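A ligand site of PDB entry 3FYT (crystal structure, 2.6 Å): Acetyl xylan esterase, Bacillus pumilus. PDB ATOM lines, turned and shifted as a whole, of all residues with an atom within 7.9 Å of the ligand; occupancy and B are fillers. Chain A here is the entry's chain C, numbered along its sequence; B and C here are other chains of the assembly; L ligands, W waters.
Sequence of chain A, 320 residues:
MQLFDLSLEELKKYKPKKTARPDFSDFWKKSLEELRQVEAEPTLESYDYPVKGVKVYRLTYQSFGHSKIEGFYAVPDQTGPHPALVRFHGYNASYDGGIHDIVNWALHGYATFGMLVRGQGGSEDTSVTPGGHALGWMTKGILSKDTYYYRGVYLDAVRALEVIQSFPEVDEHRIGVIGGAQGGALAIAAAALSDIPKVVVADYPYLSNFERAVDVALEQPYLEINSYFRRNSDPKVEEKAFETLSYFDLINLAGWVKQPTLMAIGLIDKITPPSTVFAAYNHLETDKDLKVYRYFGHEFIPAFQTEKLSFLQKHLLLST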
ATOM      1  N   TYR A 295       7.515  -9.166 -29.062  1.00  0.00           N
ATOM      2  CA  TYR A 295       7.025 -10.188 -28.158  1.00  0.00           C
ATOM      3  C   TYR A 295       8.022 -11.195 -27.626  1.00  0.00           C
ATOM      4  O   TYR A 295       7.620 -12.242 -27.112  1.00  0.00           O
ATOM      5  CB  TYR A 295       5.858 -10.904 -28.844  1.00  0.00           C
ATOM      6  CG  TYR A 295       4.764  -9.963 -29.287  1.00  0.00           C
ATOM      7  CD1 TYR A 295       3.917  -9.366 -28.351  1.00  0.00           C
ATOM      8  CD2 TYR A 295       4.591  -9.631 -30.628  1.00  0.00           C
ATOM      9  CE1 TYR A 295       2.930  -8.465 -28.750  1.00  0.00           C
ATOM     10  CE2 TYR A 295       3.609  -8.730 -31.036  1.00  0.00           C
ATOM     11  CZ  TYR A 295       2.778  -8.158 -30.092  1.00  0.00           C
ATOM     12  OH  TYR A 295       1.788  -7.291 -30.513  1.00  0.00           O
ATOM     13  N   PHE A 296       9.311 -10.891 -27.741  1.00  0.00           N
ATOM     14  CA  PHE A 296      10.337 -11.795 -27.244  1.00  0.00           C
ATOM     15  C   PHE A 296      11.271 -11.158 -26.235  1.00  0.00           C
ATOM     16  O   PHE A 296      11.454  -9.934 -26.218  1.00  0.00           O
ATOM     17  CB  PHE A 296      11.170 -12.369 -28.400  1.00  0.00           C
ATOM     18  CG  PHE A 296      10.432 -13.409 -29.192  1.00  0.00           C
ATOM     19  CD1 PHE A 296       9.528 -13.041 -30.182  1.00  0.00           C
ATOM     20  CD2 PHE A 296      10.655 -14.763 -28.946  1.00  0.00           C
ATOM     21  CE1 PHE A 296       8.836 -14.005 -30.910  1.00  0.00           C
ATOM     22  CE2 PHE A 296       9.966 -15.749 -29.672  1.00  0.00           C
ATOM     23  CZ  PHE A 296       9.060 -15.367 -30.653  1.00  0.00           C
ATOM     24  N   GLY A 297      11.852 -11.986 -25.370  1.00  0.00           N
ATOM     25  CA  GLY A 297      12.767 -11.510 -24.362  1.00  0.00           C
ATOM     26  C   GLY A 297      14.148 -12.100 -24.542  1.00  0.00           C
ATOM     27  O   GLY A 297      14.599 -12.320 -25.659  1.00  0.00           O
ATOM     28  N   HIS A 298      14.823 -12.384 -23.435  1.00  0.00           N
ATOM     29  CA  HIS A 298      16.157 -12.956 -23.484  1.00  0.00           C
ATOM     30  C   HIS A 298      15.979 -14.438 -23.776  1.00  0.00           C
ATOM     31  O   HIS A 298      16.041 -15.270 -22.866  1.00  0.00           O
ATOM     32  CB  HIS A 298      16.852 -12.784 -22.145  1.00  0.00           C
ATOM     33  CG  HIS A 298      18.339 -12.893 -22.208  1.00  0.00           C
ATOM     34  ND1 HIS A 298      19.131 -11.896 -22.717  1.00  0.00           N
ATOM     35  CD2 HIS A 298      19.179 -13.872 -21.799  1.00  0.00           C
ATOM     36  CE1 HIS A 298      20.406 -12.240 -22.616  1.00  0.00           C
ATOM     37  NE2 HIS A 298      20.460 -13.440 -22.060  1.00  0.00           N
ATOM     38  N   GLU A 299      15.786 -14.772 -25.038  1.00  0.00           N
ATOM     39  CA  GLU A 299      15.574 -16.160 -25.418  1.00  0.00           C
ATOM     40  C   GLU A 299      15.837 -16.382 -26.896  1.00  0.00           C
ATOM     41  O   GLU A 299      16.117 -15.452 -27.653  1.00  0.00           O
ATOM     42  CB  GLU A 299      14.122 -16.522 -25.112  1.00  0.00           C
ATOM     43  CG  GLU A 299      13.133 -15.778 -26.007  1.00  0.00           C
ATOM     44  CD  GLU A 299      11.706 -15.728 -25.464  1.00  0.00           C
ATOM     45  OE1 GLU A 299      11.148 -16.802 -25.127  1.00  0.00           O
ATOM     46  OE2 GLU A 299      11.156 -14.610 -25.379  1.00  0.00           O
ATOM     47  N   PHE A 300      15.728 -17.642 -27.310  1.00  0.00           N
ATOM     48  CA  PHE A 300      15.905 -18.010 -28.700  1.00  0.00           C
ATOM     49  C   PHE A 300      14.763 -17.401 -29.529  1.00  0.00           C
ATOM     50  O   PHE A 300      13.597 -17.644 -29.255  1.00  0.00           O
ATOM     51  CB  PHE A 300      15.873 -19.534 -28.850  1.00  0.00           C
ATOM     52  CG  PHE A 300      15.843 -20.004 -30.292  1.00  0.00           C
ATOM     53  CD1 PHE A 300      16.973 -19.905 -31.102  1.00  0.00           C
ATOM     54  CD2 PHE A 300      14.668 -20.501 -30.837  1.00  0.00           C
ATOM     55  CE1 PHE A 300      16.925 -20.296 -32.434  1.00  0.00           C
ATOM     56  CE2 PHE A 300      14.620 -20.892 -32.169  1.00  0.00           C
ATOM     57  CZ  PHE A 300      15.745 -20.792 -32.969  1.00  0.00           C
ATOM     58  N   ILE A 301      15.103 -16.624 -30.540  1.00  0.00           N
ATOM     59  CA  ILE A 301      14.072 -16.011 -31.382  1.00  0.00           C
ATOM     60  C   ILE A 301      14.110 -16.629 -32.772  1.00  0.00           C
ATOM     61  O   ILE A 301      14.973 -16.293 -33.591  1.00  0.00           O
ATOM     62  CB  ILE A 301      14.277 -14.493 -31.481  1.00  0.00           C
ATOM     63  CG1 ILE A 301      14.439 -13.901 -30.068  1.00  0.00           C
ATOM     64  CG2 ILE A 301      13.090 -13.860 -32.166  1.00  0.00           C
ATOM     65  CD1 ILE A 301      14.807 -12.427 -30.062  1.00  0.00           C
ATOM     66  N   PRO A 302      13.169 -17.551 -33.056  1.00  0.00           N
ATOM     67  CA  PRO A 302      13.058 -18.249 -34.337  1.00  0.00           C
ATOM     68  C   PRO A 302      13.257 -17.357 -35.568  1.00  0.00           C
ATOM     69  O   PRO A 302      14.101 -17.640 -36.421  1.00  0.00           O
ATOM     70  CB  PRO A 302      11.661 -18.849 -34.270  1.00  0.00           C
ATOM     71  CG  PRO A 302      11.530 -19.178 -32.834  1.00  0.00           C
ATOM     72  CD  PRO A 302      12.055 -17.934 -32.169  1.00  0.00           C
ATOM     73  N   ALA A 303      12.485 -16.277 -35.647  1.00  0.00           N
ATOM     74  CA  ALA A 303      12.572 -15.370 -36.777  1.00  0.00           C
ATOM     75  C   ALA A 303      13.974 -14.809 -36.995  1.00  0.00           C
ATOM     76  O   ALA A 303      14.420 -14.676 -38.122  1.00  0.00           O
ATOM     77  CB  ALA A 303      11.586 -14.220 -36.597  1.00  0.00           C
ATOM     78  N   ASN B  92       1.381 -27.370 -27.672  1.00  0.00           N
ATOM     79  CA  ASN B  92       1.368 -25.918 -27.775  1.00  0.00           C
ATOM     80  C   ASN B  92       2.795 -25.374 -27.778  1.00  0.00           C
ATOM     81  O   ASN B  92       3.040 -24.228 -27.403  1.00  0.00           O
ATOM     82  CB  ASN B  92       0.562 -25.334 -26.606  1.00  0.00           C
ATOM     83  CG  ASN B  92       0.449 -23.824 -26.649  1.00  0.00           C
ATOM     84  OD1 ASN B  92      -0.025 -23.254 -27.627  1.00  0.00           O
ATOM     85  ND2 ASN B  92       0.847 -23.167 -25.571  1.00  0.00           N
ATOM     86  N   ALA B  93       3.737 -26.201 -28.220  1.00  0.00           N
ATOM     87  CA  ALA B  93       5.141 -25.817 -28.249  1.00  0.00           C
ATOM     88  C   ALA B  93       5.739 -25.716 -29.657  1.00  0.00           C
ATOM     89  O   ALA B  93       6.908 -26.041 -29.866  1.00  0.00           O
ATOM     90  CB  ALA B  93       5.944 -26.788 -27.413  1.00  0.00           C
ATOM     91  N   SER B  94       4.947 -25.266 -30.618  1.00  0.00           N
ATOM     92  CA  SER B  94       5.442 -25.150 -31.976  1.00  0.00           C
ATOM     93  C   SER B  94       5.511 -23.693 -32.417  1.00  0.00           C
ATOM     94  O   SER B  94       4.509 -22.973 -32.402  1.00  0.00           O
ATOM     95  CB  SER B  94       4.529 -25.928 -32.934  1.00  0.00           C
ATOM     96  OG  SER B  94       5.049 -25.880 -34.254  1.00  0.00           O
ATOM     97  N   TYR B  95       6.704 -23.259 -32.788  1.00  0.00           N
ATOM     98  CA  TYR B  95       6.913 -21.890 -33.235  1.00  0.00           C
ATOM     99  C   TYR B  95       7.376 -21.915 -34.691  1.00  0.00           C
ATOM    100  O   TYR B  95       8.377 -22.554 -35.024  1.00  0.00           O
ATOM    101  CB  TYR B  95       7.979 -21.190 -32.386  1.00  0.00           C
ATOM    102  CG  TYR B  95       7.615 -20.988 -30.924  1.00  0.00           C
ATOM    103  CD1 TYR B  95       7.378 -22.070 -30.082  1.00  0.00           C
ATOM    104  CD2 TYR B  95       7.527 -19.692 -30.375  1.00  0.00           C
ATOM    105  CE1 TYR B  95       7.070 -21.887 -28.736  1.00  0.00           C
ATOM    106  CE2 TYR B  95       7.226 -19.503 -29.026  1.00  0.00           C
ATOM    107  CZ  TYR B  95       7.000 -20.601 -28.211  1.00  0.00           C
ATOM    108  OH  TYR B  95       6.714 -20.429 -26.865  1.00  0.00           O
ATOM    109  N   ASP B 101      14.372 -26.880 -37.067  1.00  0.00           N
ATOM    110  CA  ASP B 101      14.669 -28.238 -36.617  1.00  0.00           C
ATOM    111  C   ASP B 101      14.522 -29.183 -37.803  1.00  0.00           C
ATOM    112  O   ASP B 101      15.355 -30.071 -38.016  1.00  0.00           O
ATOM    113  CB  ASP B 101      13.697 -28.686 -35.511  1.00  0.00           C
ATOM    114  CG  ASP B 101      13.931 -27.952 -34.205  1.00  0.00           C
ATOM    115  OD1 ASP B 101      14.992 -28.163 -33.569  1.00  0.00           O
ATOM    116  OD2 ASP B 101      13.043 -27.154 -33.802  1.00  0.00           O
ATOM    117  N   ARG C 230       3.995 -14.884 -31.024  1.00  0.00           N
ATOM    118  CA  ARG C 230       5.308 -15.446 -30.771  1.00  0.00           C
ATOM    119  C   ARG C 230       5.479 -16.682 -31.640  1.00  0.00           C
ATOM    120  O   ARG C 230       6.562 -16.941 -32.163  1.00  0.00           O
ATOM    121  CB  ARG C 230       5.448 -15.812 -29.299  1.00  0.00           C
ATOM    122  CG  ARG C 230       5.655 -14.619 -28.353  1.00  0.00           C
ATOM    123  CD  ARG C 230       5.436 -15.062 -26.909  1.00  0.00           C
ATOM    124  NE  ARG C 230       6.354 -16.124 -26.524  1.00  0.00           N
ATOM    125  CZ  ARG C 230       7.647 -15.933 -26.241  1.00  0.00           C
ATOM    126  NH1 ARG C 230       8.161 -14.710 -26.295  1.00  0.00           N
ATOM    127  NH2 ARG C 230       8.415 -16.961 -25.944  1.00  0.00           N
ATOM    128  N   ARG C 231       4.411 -17.443 -31.805  1.00  0.00           N
ATOM    129  CA  ARG C 231       4.439 -18.665 -32.589  1.00  0.00           C
ATOM    130  C   ARG C 231       4.267 -18.429 -34.093  1.00  0.00           C
ATOM    131  O   ARG C 231       4.549 -19.333 -34.890  1.00  0.00           O
ATOM    132  CB  ARG C 231       3.358 -19.623 -32.081  1.00  0.00           C
ATOM    133  CG  ARG C 231       3.594 -20.082 -30.656  1.00  0.00           C
ATOM    134  CD  ARG C 231       2.354 -20.681 -30.010  1.00  0.00           C
ATOM    135  NE  ARG C 231       2.685 -21.344 -28.764  1.00  0.00           N
ATOM    136  CZ  ARG C 231       3.181 -20.738 -27.690  1.00  0.00           C
ATOM    137  NH1 ARG C 231       3.397 -19.418 -27.706  1.00  0.00           N
ATOM    138  NH2 ARG C 231       3.487 -21.435 -26.599  1.00  0.00           N
HETATM  139  O1  LIG L   1      10.161 -23.822 -26.876  1.00  0.00           O
HETATM  140  C1  LIG L   1      10.207 -22.478 -27.279  1.00  0.00           C
HETATM  141  C2  LIG L   1      10.857 -21.713 -26.137  1.00  0.00           C
HETATM  142  C3  LIG L   1      10.944 -20.239 -26.527  1.00  0.00           C
HETATM  143  C4  LIG L   1      11.725 -20.092 -27.823  1.00  0.00           C
HETATM  144  C5  LIG L   1      11.030 -20.959 -28.893  1.00  0.00           C
HETATM  145  O2  LIG L   1      10.098 -21.797 -24.911  1.00  0.00           O
HETATM  146  O3  LIG L   1      11.585 -19.448 -25.502  1.00  0.00           O
HETATM  147  O4  LIG L   1      11.719 -18.753 -28.251  1.00  0.00           O
HETATM  148  O5  LIG L   1      10.977 -22.353 -28.446  1.00  0.00           O
HETATM  149  O   HOH W   1      14.740 -19.902 -24.925  1.00  0.00           O
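CE2 of Phe 296 touches O4 of the ligand, at 3.8 Å. Tyr 95 of chain B touches the ligand (CE1 to C1, 3.5 Å). Hydrophobic or aromatic side chains within 4 Å of the ligand: Phe 296 and Tyr 95 of chain B. Of the 16 residues printed, 4 come within 4 Å of the ligand. The nearest printed residue that does not touch the ligand is Pro 302 (4.02 Å).
O of Phe 300 sits at hydrogen-bond distance from O4 of the ligand, at 2.4 Å. OE1 of Glu 299 is in hydrogen-bond range of O3 of the ligand (2.7 Å).
Water W1 lies within hydrogen-bond range of an oxygen (O3) of the ligand (3.2 Å) and the backbone NH (N) of Phe 300 (3.4 Å).
The guanidinium group of Arg 230 of chain C is in salt-bridge range of the side-chain carboxylate of Glu 299 (2.9 Å). The side-chain carboxylate of Glu 299 is in hydrogen-bond range of the backbone NH of Gly 297, at 2.7 Å. OH of Tyr 95 of chain B sits at hydrogen-bond distance from NH2 of Arg 231 of chain C (3.4 Å).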
